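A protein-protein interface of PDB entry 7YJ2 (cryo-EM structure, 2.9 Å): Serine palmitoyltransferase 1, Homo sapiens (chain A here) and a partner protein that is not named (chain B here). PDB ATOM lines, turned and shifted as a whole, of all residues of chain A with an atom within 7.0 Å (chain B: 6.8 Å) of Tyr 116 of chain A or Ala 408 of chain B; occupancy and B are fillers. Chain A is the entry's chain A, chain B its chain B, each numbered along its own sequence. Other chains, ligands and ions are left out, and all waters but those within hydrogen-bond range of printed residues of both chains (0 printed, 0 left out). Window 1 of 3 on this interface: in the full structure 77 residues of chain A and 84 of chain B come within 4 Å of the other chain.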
ATOM      1  N   ILE A 113      22.185   8.817 -14.717  1.00  0.00           N
ATOM      2  CA  ILE A 113      22.293   7.855 -13.624  1.00  0.00           C
ATOM      3  C   ILE A 113      20.905   7.495 -13.120  1.00  0.00           C
ATOM      4  O   ILE A 113      20.024   8.353 -13.034  1.00  0.00           O
ATOM      5  CB  ILE A 113      23.175   8.365 -12.469  1.00  0.00           C
ATOM      6  CG1 ILE A 113      22.665   9.680 -11.912  1.00  0.00           C
ATOM      7  CG2 ILE A 113      24.617   8.492 -12.898  1.00  0.00           C
ATOM      8  CD1 ILE A 113      23.323  10.063 -10.623  1.00  0.00           C
ATOM      9  N   TYR A 114      20.710   6.211 -12.831  1.00  0.00           N
ATOM     10  CA  TYR A 114      19.519   5.667 -12.205  1.00  0.00           C
ATOM     11  C   TYR A 114      19.822   5.361 -10.744  1.00  0.00           C
ATOM     12  O   TYR A 114      20.970   5.366 -10.313  1.00  0.00           O
ATOM     13  CB  TYR A 114      19.054   4.410 -12.934  1.00  0.00           C
ATOM     14  CG  TYR A 114      18.364   4.659 -14.250  1.00  0.00           C
ATOM     15  CD1 TYR A 114      17.002   4.498 -14.370  1.00  0.00           C
ATOM     16  CD2 TYR A 114      19.080   5.025 -15.377  1.00  0.00           C
ATOM     17  CE1 TYR A 114      16.368   4.717 -15.552  1.00  0.00           C
ATOM     18  CE2 TYR A 114      18.449   5.249 -16.569  1.00  0.00           C
ATOM     19  CZ  TYR A 114      17.090   5.089 -16.651  1.00  0.00           C
ATOM     20  OH  TYR A 114      16.441   5.302 -17.835  1.00  0.00           O
ATOM     21  N   SER A 115      18.781   5.083  -9.969  1.00  0.00           N
ATOM     22  CA  SER A 115      18.936   4.812  -8.547  1.00  0.00           C
ATOM     23  C   SER A 115      18.904   3.328  -8.226  1.00  0.00           C
ATOM     24  O   SER A 115      18.903   2.957  -7.053  1.00  0.00           O
ATOM     25  CB  SER A 115      17.862   5.539  -7.745  1.00  0.00           C
ATOM     26  OG  SER A 115      16.585   5.013  -8.009  1.00  0.00           O
ATOM     27  N   TYR A 116      18.890   2.474  -9.237  1.00  0.00           N
ATOM     28  CA  TYR A 116      18.793   1.040  -9.058  1.00  0.00           C
ATOM     29  C   TYR A 116      19.451   0.376 -10.252  1.00  0.00           C
ATOM     30  O   TYR A 116      19.179   0.740 -11.394  1.00  0.00           O
ATOM     31  CB  TYR A 116      17.336   0.625  -8.934  1.00  0.00           C
ATOM     32  CG  TYR A 116      17.067  -0.664  -8.209  1.00  0.00           C
ATOM     33  CD1 TYR A 116      17.477  -0.844  -6.913  1.00  0.00           C
ATOM     34  CD2 TYR A 116      16.330  -1.667  -8.801  1.00  0.00           C
ATOM     35  CE1 TYR A 116      17.225  -2.003  -6.258  1.00  0.00           C
ATOM     36  CE2 TYR A 116      16.064  -2.823  -8.144  1.00  0.00           C
ATOM     37  CZ  TYR A 116      16.505  -2.984  -6.869  1.00  0.00           C
ATOM     38  OH  TYR A 116      16.233  -4.145  -6.200  1.00  0.00           O
ATOM     39  N   GLY A 117      20.321  -0.587  -9.983  1.00  0.00           N
ATOM     40  CA  GLY A 117      21.091  -1.214 -11.034  1.00  0.00           C
ATOM     41  C   GLY A 117      20.302  -2.033 -12.021  1.00  0.00           C
ATOM     42  O   GLY A 117      20.683  -2.100 -13.187  1.00  0.00           O
ATOM     43  N   PHE A 118      19.231  -2.680 -11.577  1.00  0.00           N
ATOM     44  CA  PHE A 118      18.392  -3.499 -12.438  1.00  0.00           C
ATOM     45  C   PHE A 118      17.513  -2.678 -13.361  1.00  0.00           C
ATOM     46  O   PHE A 118      17.265  -3.101 -14.489  1.00  0.00           O
ATOM     47  CB  PHE A 118      17.509  -4.417 -11.577  1.00  0.00           C
ATOM     48  CG  PHE A 118      16.768  -5.482 -12.347  1.00  0.00           C
ATOM     49  CD1 PHE A 118      17.194  -6.793 -12.318  1.00  0.00           C
ATOM     50  CD2 PHE A 118      15.616  -5.183 -13.061  1.00  0.00           C
ATOM     51  CE1 PHE A 118      16.508  -7.774 -13.005  1.00  0.00           C
ATOM     52  CE2 PHE A 118      14.936  -6.160 -13.758  1.00  0.00           C
ATOM     53  CZ  PHE A 118      15.382  -7.455 -13.726  1.00  0.00           C
ATOM     54  N   ALA A 119      17.056  -1.513 -12.920  1.00  0.00           N
ATOM     55  CA  ALA A 119      16.103  -0.700 -13.653  1.00  0.00           C
ATOM     56  C   ALA A 119      16.758   0.147 -14.725  1.00  0.00           C
ATOM     57  O   ALA A 119      16.064   0.868 -15.439  1.00  0.00           O
ATOM     58  CB  ALA A 119      15.338   0.197 -12.687  1.00  0.00           C
ATOM     59  N   THR A 120      18.073   0.081 -14.854  1.00  0.00           N
ATOM     60  CA  THR A 120      18.776   0.879 -15.840  1.00  0.00           C
ATOM     61  C   THR A 120      18.562   0.369 -17.252  1.00  0.00           C
ATOM     62  O   THR A 120      18.144   1.132 -18.123  1.00  0.00           O
ATOM     63  CB  THR A 120      20.262   0.908 -15.508  1.00  0.00           C
ATOM     64  OG1 THR A 120      20.423   1.392 -14.176  1.00  0.00           O
ATOM     65  CG2 THR A 120      21.001   1.810 -16.445  1.00  0.00           C
ATOM     66  N   ILE A 121      18.830  -0.917 -17.495  1.00  0.00           N
ATOM     67  CA  ILE A 121      18.658  -1.495 -18.824  1.00  0.00           C
ATOM     68  C   ILE A 121      17.257  -2.046 -19.021  1.00  0.00           C
ATOM     69  O   ILE A 121      16.877  -2.355 -20.157  1.00  0.00           O
ATOM     70  CB  ILE A 121      19.731  -2.575 -19.078  1.00  0.00           C
ATOM     71  CG1 ILE A 121      19.856  -2.914 -20.562  1.00  0.00           C
ATOM     72  CG2 ILE A 121      19.440  -3.812 -18.301  1.00  0.00           C
ATOM     73  CD1 ILE A 121      20.316  -1.773 -21.422  1.00  0.00           C
ATOM     74  N   ALA A 255      25.758   0.312 -17.775  1.00  0.00           N
ATOM     75  CA  ALA A 255      26.507  -0.367 -16.730  1.00  0.00           C
ATOM     76  C   ALA A 255      25.816  -0.076 -15.410  1.00  0.00           C
ATOM     77  O   ALA A 255      24.902   0.742 -15.341  1.00  0.00           O
ATOM     78  CB  ALA A 255      27.966   0.082 -16.700  1.00  0.00           C
ATOM     79  N   ASN A 256      26.252  -0.758 -14.362  1.00  0.00           N
ATOM     80  CA  ASN A 256      25.757  -0.477 -13.027  1.00  0.00           C
ATOM     81  C   ASN A 256      26.918  -0.059 -12.140  1.00  0.00           C
ATOM     82  O   ASN A 256      28.080  -0.336 -12.435  1.00  0.00           O
ATOM     83  CB  ASN A 256      24.996  -1.666 -12.428  1.00  0.00           C
ATOM     84  CG  ASN A 256      25.825  -2.904 -12.318  1.00  0.00           C
ATOM     85  OD1 ASN A 256      27.042  -2.866 -12.404  1.00  0.00           O
ATOM     86  ND2 ASN A 256      25.163  -4.028 -12.126  1.00  0.00           N
ATOM     87  N   GLU A 258      27.539  -0.963  -9.075  1.00  0.00           N
ATOM     88  CA  GLU A 258      27.429  -1.878  -7.959  1.00  0.00           C
ATOM     89  C   GLU A 258      28.541  -2.906  -7.867  1.00  0.00           C
ATOM     90  O   GLU A 258      28.742  -3.461  -6.785  1.00  0.00           O
ATOM     91  CB  GLU A 258      26.082  -2.604  -8.020  1.00  0.00           C
ATOM     92  CG  GLU A 258      24.932  -1.683  -7.743  1.00  0.00           C
ATOM     93  CD  GLU A 258      23.596  -2.265  -8.088  1.00  0.00           C
ATOM     94  OE1 GLU A 258      23.556  -3.267  -8.823  1.00  0.00           O
ATOM     95  OE2 GLU A 258      22.579  -1.721  -7.613  1.00  0.00           O
ATOM     96  N   ILE A 264      25.628   1.810  -5.329  1.00  0.00           N
ATOM     97  CA  ILE A 264      24.271   1.505  -5.760  1.00  0.00           C
ATOM     98  C   ILE A 264      23.955   2.297  -7.020  1.00  0.00           C
ATOM     99  O   ILE A 264      24.316   3.472  -7.123  1.00  0.00           O
ATOM    100  CB  ILE A 264      23.255   1.822  -4.644  1.00  0.00           C
ATOM    101  CG1 ILE A 264      23.646   1.106  -3.352  1.00  0.00           C
ATOM    102  CG2 ILE A 264      21.864   1.441  -5.057  1.00  0.00           C
ATOM    103  CD1 ILE A 264      23.407  -0.374  -3.362  1.00  0.00           C
ATOM    104  N   GLY A 265      23.299   1.661  -7.978  1.00  0.00           N
ATOM    105  CA  GLY A 265      22.722   2.354  -9.112  1.00  0.00           C
ATOM    106  C   GLY A 265      23.331   1.915 -10.432  1.00  0.00           C
ATOM    107  O   GLY A 265      24.227   1.077 -10.498  1.00  0.00           O
ATOM    108  N   GLY A 266      22.818   2.512 -11.506  1.00  0.00           N
ATOM    109  CA  GLY A 266      23.358   2.276 -12.826  1.00  0.00           C
ATOM    110  C   GLY A 266      23.425   3.562 -13.623  1.00  0.00           C
ATOM    111  O   GLY A 266      22.915   4.590 -13.202  1.00  0.00           O
ATOM    112  N   PHE A 267      24.058   3.482 -14.788  1.00  0.00           N
ATOM    113  CA  PHE A 267      24.174   4.659 -15.636  1.00  0.00           C
ATOM    114  C   PHE A 267      24.226   4.246 -17.098  1.00  0.00           C
ATOM    115  O   PHE A 267      24.663   3.148 -17.433  1.00  0.00           O
ATOM    116  CB  PHE A 267      25.401   5.498 -15.260  1.00  0.00           C
ATOM    117  CG  PHE A 267      26.701   4.934 -15.739  1.00  0.00           C
ATOM    118  CD1 PHE A 267      27.360   3.976 -15.010  1.00  0.00           C
ATOM    119  CD2 PHE A 267      27.276   5.385 -16.899  1.00  0.00           C
ATOM    120  CE1 PHE A 267      28.547   3.463 -15.447  1.00  0.00           C
ATOM    121  CE2 PHE A 267      28.458   4.874 -17.334  1.00  0.00           C
ATOM    122  CZ  PHE A 267      29.094   3.914 -16.608  1.00  0.00           C
ATOM    123  N   GLY A 284      11.776   4.333 -14.805  1.00  0.00           N
ATOM    124  CA  GLY A 284      12.425   4.345 -13.516  1.00  0.00           C
ATOM    125  C   GLY A 284      13.235   5.576 -13.212  1.00  0.00           C
ATOM    126  O   GLY A 284      13.749   5.697 -12.099  1.00  0.00           O
ATOM    127  N   SER A 288      10.497   7.710  -9.804  1.00  0.00           N
ATOM    128  CA  SER A 288      11.141   7.141  -8.635  1.00  0.00           C
ATOM    129  C   SER A 288      12.009   8.205  -7.993  1.00  0.00           C
ATOM    130  O   SER A 288      12.489   9.117  -8.667  1.00  0.00           O
ATOM    131  CB  SER A 288      11.972   5.914  -9.002  1.00  0.00           C
ATOM    132  OG  SER A 288      12.225   5.107  -7.868  1.00  0.00           O
ATOM    133  N   ALA A 289      12.192   8.084  -6.687  1.00  0.00           N
ATOM    134  CA  ALA A 289      13.098   8.965  -5.977  1.00  0.00           C
ATOM    135  C   ALA A 289      14.522   8.766  -6.467  1.00  0.00           C
ATOM    136  O   ALA A 289      14.927   7.667  -6.838  1.00  0.00           O
ATOM    137  CB  ALA A 289      13.018   8.704  -4.480  1.00  0.00           C
ATOM    138  N   LEU A 291      18.850   9.070  -6.309  1.00  0.00           N
ATOM    139  CA  LEU A 291      19.818   8.329  -5.518  1.00  0.00           C
ATOM    140  C   LEU A 291      20.198   9.106  -4.261  1.00  0.00           C
ATOM    141  O   LEU A 291      20.370  10.326  -4.331  1.00  0.00           O
ATOM    142  CB  LEU A 291      21.049   8.062  -6.383  1.00  0.00           C
ATOM    143  CG  LEU A 291      22.247   7.274  -5.877  1.00  0.00           C
ATOM    144  CD1 LEU A 291      21.890   5.832  -5.717  1.00  0.00           C
ATOM    145  CD2 LEU A 291      23.374   7.406  -6.853  1.00  0.00           C
ATOM    146  N   SER B 205      26.283  -8.126  -3.947  1.00  0.00           N
ATOM    147  CA  SER B 205      25.666  -9.365  -4.394  1.00  0.00           C
ATOM    148  C   SER B 205      24.189  -9.332  -4.052  1.00  0.00           C
ATOM    149  O   SER B 205      23.683  -8.358  -3.501  1.00  0.00           O
ATOM    150  CB  SER B 205      26.334 -10.582  -3.769  1.00  0.00           C
ATOM    151  OG  SER B 205      25.761 -11.777  -4.258  1.00  0.00           O
ATOM    152  N   THR B 206      23.509 -10.427  -4.366  1.00  0.00           N
ATOM    153  CA  THR B 206      22.067 -10.534  -4.219  1.00  0.00           C
ATOM    154  C   THR B 206      21.698 -11.250  -2.924  1.00  0.00           C
ATOM    155  O   THR B 206      22.515 -11.913  -2.293  1.00  0.00           O
ATOM    156  CB  THR B 206      21.459 -11.254  -5.421  1.00  0.00           C
ATOM    157  OG1 THR B 206      22.157 -12.475  -5.662  1.00  0.00           O
ATOM    158  CG2 THR B 206      21.570 -10.405  -6.643  1.00  0.00           C
ATOM    159  N   ARG B 207      20.436 -11.096  -2.529  1.00  0.00           N
ATOM    160  CA  ARG B 207      19.969 -11.662  -1.268  1.00  0.00           C
ATOM    161  C   ARG B 207      20.127 -13.168  -1.228  1.00  0.00           C
ATOM    162  O   ARG B 207      20.221 -13.750  -0.149  1.00  0.00           O
ATOM    163  CB  ARG B 207      18.504 -11.309  -1.038  1.00  0.00           C
ATOM    164  CG  ARG B 207      18.285  -9.957  -0.441  1.00  0.00           C
ATOM    165  CD  ARG B 207      18.862  -9.865   0.941  1.00  0.00           C
ATOM    166  NE  ARG B 207      18.004 -10.501   1.925  1.00  0.00           N
ATOM    167  CZ  ARG B 207      16.862  -9.993   2.357  1.00  0.00           C
ATOM    168  NH1 ARG B 207      16.149 -10.643   3.255  1.00  0.00           N
ATOM    169  NH2 ARG B 207      16.434  -8.838   1.894  1.00  0.00           N
ATOM    170  N   GLN B 208      20.138 -13.814  -2.381  1.00  0.00           N
ATOM    171  CA  GLN B 208      20.155 -15.261  -2.436  1.00  0.00           C
ATOM    172  C   GLN B 208      21.549 -15.846  -2.563  1.00  0.00           C
ATOM    173  O   GLN B 208      21.707 -17.044  -2.332  1.00  0.00           O
ATOM    174  CB  GLN B 208      19.287 -15.759  -3.591  1.00  0.00           C
ATOM    175  CG  GLN B 208      17.913 -16.217  -3.169  1.00  0.00           C
ATOM    176  CD  GLN B 208      17.135 -16.809  -4.305  1.00  0.00           C
ATOM    177  OE1 GLN B 208      17.701 -17.160  -5.324  1.00  0.00           O
ATOM    178  NE2 GLN B 208      15.838 -16.944  -4.132  1.00  0.00           N
ATOM    179  N   TYR B 235      13.176  -4.484  -0.009  1.00  0.00           N
ATOM    180  CA  TYR B 235      13.724  -4.633  -1.354  1.00  0.00           C
ATOM    181  C   TYR B 235      14.819  -3.638  -1.718  1.00  0.00           C
ATOM    182  O   TYR B 235      15.897  -4.064  -2.137  1.00  0.00           O
ATOM    183  CB  TYR B 235      12.586  -4.580  -2.366  1.00  0.00           C
ATOM    184  CG  TYR B 235      11.689  -5.766  -2.217  1.00  0.00           C
ATOM    185  CD1 TYR B 235      12.112  -7.022  -2.592  1.00  0.00           C
ATOM    186  CD2 TYR B 235      10.438  -5.637  -1.674  1.00  0.00           C
ATOM    187  CE1 TYR B 235      11.309  -8.105  -2.441  1.00  0.00           C
ATOM    188  CE2 TYR B 235       9.627  -6.711  -1.528  1.00  0.00           C
ATOM    189  CZ  TYR B 235      10.067  -7.943  -1.908  1.00  0.00           C
ATOM    190  OH  TYR B 235       9.243  -9.021  -1.758  1.00  0.00           O
ATOM    191  N   GLY B 236      14.592  -2.343  -1.628  1.00  0.00           N
ATOM    192  CA  GLY B 236      15.655  -1.462  -2.071  1.00  0.00           C
ATOM    193  C   GLY B 236      15.263  -0.440  -3.113  1.00  0.00           C
ATOM    194  O   GLY B 236      15.977   0.541  -3.311  1.00  0.00           O
ATOM    195  N   MET B 237      14.141  -0.646  -3.787  1.00  0.00           N
ATOM    196  CA  MET B 237      13.581   0.395  -4.638  1.00  0.00           C
ATOM    197  C   MET B 237      12.074   0.308  -4.526  1.00  0.00           C
ATOM    198  O   MET B 237      11.522  -0.790  -4.588  1.00  0.00           O
ATOM    199  CB  MET B 237      14.025   0.230  -6.071  1.00  0.00           C
ATOM    200  CG  MET B 237      13.675   1.384  -6.967  1.00  0.00           C
ATOM    201  SD  MET B 237      13.797   0.935  -8.694  1.00  0.00           S
ATOM    202  CE  MET B 237      13.838   2.538  -9.440  1.00  0.00           C
ATOM    203  N   ALA B 240      10.460  -0.763  -7.886  1.00  0.00           N
ATOM    204  CA  ALA B 240      10.709  -2.150  -8.240  1.00  0.00           C
ATOM    205  C   ALA B 240      10.080  -3.147  -7.274  1.00  0.00           C
ATOM    206  O   ALA B 240      10.152  -4.350  -7.515  1.00  0.00           O
ATOM    207  CB  ALA B 240      12.209  -2.402  -8.331  1.00  0.00           C
ATOM    208  N   MET B 244       8.395  -5.999  -9.895  1.00  0.00           N
ATOM    209  CA  MET B 244       9.146  -7.236  -9.796  1.00  0.00           C
ATOM    210  C   MET B 244       8.502  -8.246  -8.857  1.00  0.00           C
ATOM    211  O   MET B 244       9.054  -9.331  -8.685  1.00  0.00           O
ATOM    212  CB  MET B 244      10.584  -6.940  -9.351  1.00  0.00           C
ATOM    213  CG  MET B 244      11.343  -6.156 -10.407  1.00  0.00           C
ATOM    214  SD  MET B 244      13.026  -5.626 -10.079  1.00  0.00           S
ATOM    215  CE  MET B 244      13.912  -7.155 -10.140  1.00  0.00           C
ATOM    216  N   HIS B 403      11.762 -11.647  -8.530  1.00  0.00           N
ATOM    217  CA  HIS B 403      12.822 -11.246  -9.439  1.00  0.00           C
ATOM    218  C   HIS B 403      13.932 -10.520  -8.696  1.00  0.00           C
ATOM    219  O   HIS B 403      15.113 -10.692  -9.008  1.00  0.00           O
ATOM    220  CB  HIS B 403      12.253 -10.369 -10.548  1.00  0.00           C
ATOM    221  CG  HIS B 403      11.148 -11.006 -11.332  1.00  0.00           C
ATOM    222  ND1 HIS B 403      10.449 -10.332 -12.309  1.00  0.00           N
ATOM    223  CD2 HIS B 403      10.630 -12.253 -11.297  1.00  0.00           C
ATOM    224  CE1 HIS B 403       9.546 -11.135 -12.838  1.00  0.00           C
ATOM    225  NE2 HIS B 403       9.632 -12.307 -12.237  1.00  0.00           N
ATOM    226  N   SER B 404      13.571  -9.700  -7.712  1.00  0.00           N
ATOM    227  CA  SER B 404      14.546  -8.898  -6.986  1.00  0.00           C
ATOM    228  C   SER B 404      15.389  -9.734  -6.044  1.00  0.00           C
ATOM    229  O   SER B 404      16.567  -9.434  -5.839  1.00  0.00           O
ATOM    230  CB  SER B 404      13.834  -7.806  -6.194  1.00  0.00           C
ATOM    231  OG  SER B 404      13.070  -6.975  -7.038  1.00  0.00           O
ATOM    232  N   ALA B 405      14.799 -10.760  -5.440  1.00  0.00           N
ATOM    233  CA  ALA B 405      15.537 -11.587  -4.498  1.00  0.00           C
ATOM    234  C   ALA B 405      16.673 -12.347  -5.173  1.00  0.00           C
ATOM    235  O   ALA B 405      17.699 -12.601  -4.543  1.00  0.00           O
ATOM    236  CB  ALA B 405      14.577 -12.555  -3.810  1.00  0.00           C
ATOM    237  N   VAL B 406      16.517 -12.704  -6.439  1.00  0.00           N
ATOM    238  CA  VAL B 406      17.489 -13.539  -7.126  1.00  0.00           C
ATOM    239  C   VAL B 406      18.339 -12.774  -8.135  1.00  0.00           C
ATOM    240  O   VAL B 406      19.460 -13.219  -8.433  1.00  0.00           O
ATOM    241  CB  VAL B 406      16.798 -14.752  -7.789  1.00  0.00           C
ATOM    242  CG1 VAL B 406      15.692 -14.315  -8.667  1.00  0.00           C
ATOM    243  CG2 VAL B 406      17.775 -15.590  -8.590  1.00  0.00           C
ATOM    244  N   TYR B 407      17.889 -11.626  -8.637  1.00  0.00           N
ATOM    245  CA  TYR B 407      18.698 -10.937  -9.634  1.00  0.00           C
ATOM    246  C   TYR B 407      19.218  -9.575  -9.202  1.00  0.00           C
ATOM    247  O   TYR B 407      20.266  -9.156  -9.682  1.00  0.00           O
ATOM    248  CB  TYR B 407      17.911 -10.797 -10.935  1.00  0.00           C
ATOM    249  CG  TYR B 407      17.712 -12.112 -11.643  1.00  0.00           C
ATOM    250  CD1 TYR B 407      18.775 -12.776 -12.226  1.00  0.00           C
ATOM    251  CD2 TYR B 407      16.470 -12.711 -11.691  1.00  0.00           C
ATOM    252  CE1 TYR B 407      18.599 -13.979 -12.846  1.00  0.00           C
ATOM    253  CE2 TYR B 407      16.287 -13.907 -12.320  1.00  0.00           C
ATOM    254  CZ  TYR B 407      17.353 -14.536 -12.891  1.00  0.00           C
ATOM    255  OH  TYR B 407      17.163 -15.733 -13.516  1.00  0.00           O
ATOM    256  N   ALA B 408      18.529  -8.868  -8.316  1.00  0.00           N
ATOM    257  CA  ALA B 408      18.912  -7.505  -7.977  1.00  0.00           C
ATOM    258  C   ALA B 408      19.636  -7.453  -6.638  1.00  0.00           C
ATOM    259  O   ALA B 408      19.339  -8.220  -5.720  1.00  0.00           O
ATOM    260  CB  ALA B 408      17.680  -6.610  -7.935  1.00  0.00           C
ATOM    261  N   THR B 409      20.587  -6.529  -6.524  1.00  0.00           N
ATOM    262  CA  THR B 409      21.381  -6.432  -5.308  1.00  0.00           C
ATOM    263  C   THR B 409      20.534  -5.901  -4.159  1.00  0.00           C
ATOM    264  O   THR B 409      19.455  -5.345  -4.355  1.00  0.00           O
ATOM    265  CB  THR B 409      22.599  -5.536  -5.513  1.00  0.00           C
ATOM    266  OG1 THR B 409      22.177  -4.180  -5.635  1.00  0.00           O
ATOM    267  CG2 THR B 409      23.338  -5.928  -6.771  1.00  0.00           C
ATOM    268  N   SER B 410      21.045  -6.070  -2.946  1.00  0.00           N
ATOM    269  CA  SER B 410      20.268  -5.832  -1.739  1.00  0.00           C
ATOM    270  C   SER B 410      20.250  -4.345  -1.388  1.00  0.00           C
ATOM    271  O   SER B 410      20.676  -3.486  -2.161  1.00  0.00           O
ATOM    272  CB  SER B 410      20.830  -6.662  -0.598  1.00  0.00           C
ATOM    273  OG  SER B 410      20.818  -8.029  -0.918  1.00  0.00           O
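OG1 of Thr 409 of chain B sits at hydrogen-bond distance from OE2 of Glu 258 of chain A, 3.2 Å away.
The backbone NH of Gly 117 of chain A is in hydrogen-bond range of the side-chain carboxylate of Glu 258 of chain A (3.5 Å).
The side-chain carboxylate (OE2) of Glu 258 of chain A is in hydrogen-bond range of the backbone NH (N) of Gly 265 of chain A (3.5 Å).
The backbone carbonyl oxygen (O) of Tyr 116 of chain A sits at hydrogen-bond distance from the side-chain hydroxyl (OG1) of Thr 120 of chain A.
The side-chain sulfur (SD) of Met 244 of chain B sits close to the side-chain hydroxyl (OG) of Ser 404 of chain B (3.3 Å).
The side-chain hydroxyl of Ser 115 of chain A sits at hydrogen-bond distance from the backbone carbonyl oxygen of Ala 289 of chain A (3.3 Å).
Ser 115 of chain A touches Met 237 of chain B (OG to CE, 3.96 Å).
Met 237 of chain B touches Tyr 116 of chain A (SD to CB, 3.6 Å).
Ala 240 of chain B touches Tyr 116 of chain A.
OH of Tyr 116 of chain A touches CB of Ala 408 of chain B, at 3.3 Å.
O of Thr 409 of chain B touches OH of Tyr 116 of chain A, 3.9 Å away.
CZ of Phe 118 of chain A touches CE of Met 244 of chain B, 3.9 Å away.
CB of Tyr 407 of chain B touches CE1 of Phe 118 of chain A, 3.9 Å away.
Met 237 of chain B touches Ser 288 of chain A.
Tyr 116 of chain A touches four residues of chain B.
Printed residues of chain A within 4 Å of Met 244 of chain B: Phe 118.
Printed residues of chain A within 4 Å of Thr 409 of chain B: Tyr 116 (3.9 Å) and Glu 258 (3.2 Å).
The nearest residue of chain A that does not touch Ala 408 of chain B is Phe 118 of chain A (4.3 Å).
Of the 20 printed residues of chain A, 5 touch a printed residue of chain B.
Hydrophobic or aromatic side chains of chain A within 4 Å of the printed part of chain B: Tyr 116 and Phe 118.
Of the 17 printed residues of chain B, 6 touch a printed residue of chain A.
Among the printed residues, 9 pairs touch across the chains.
Among the printed residues, no Asp or Glu carboxylate lies within 4 Å of a Lys or Arg side-chain nitrogen of the other chain.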
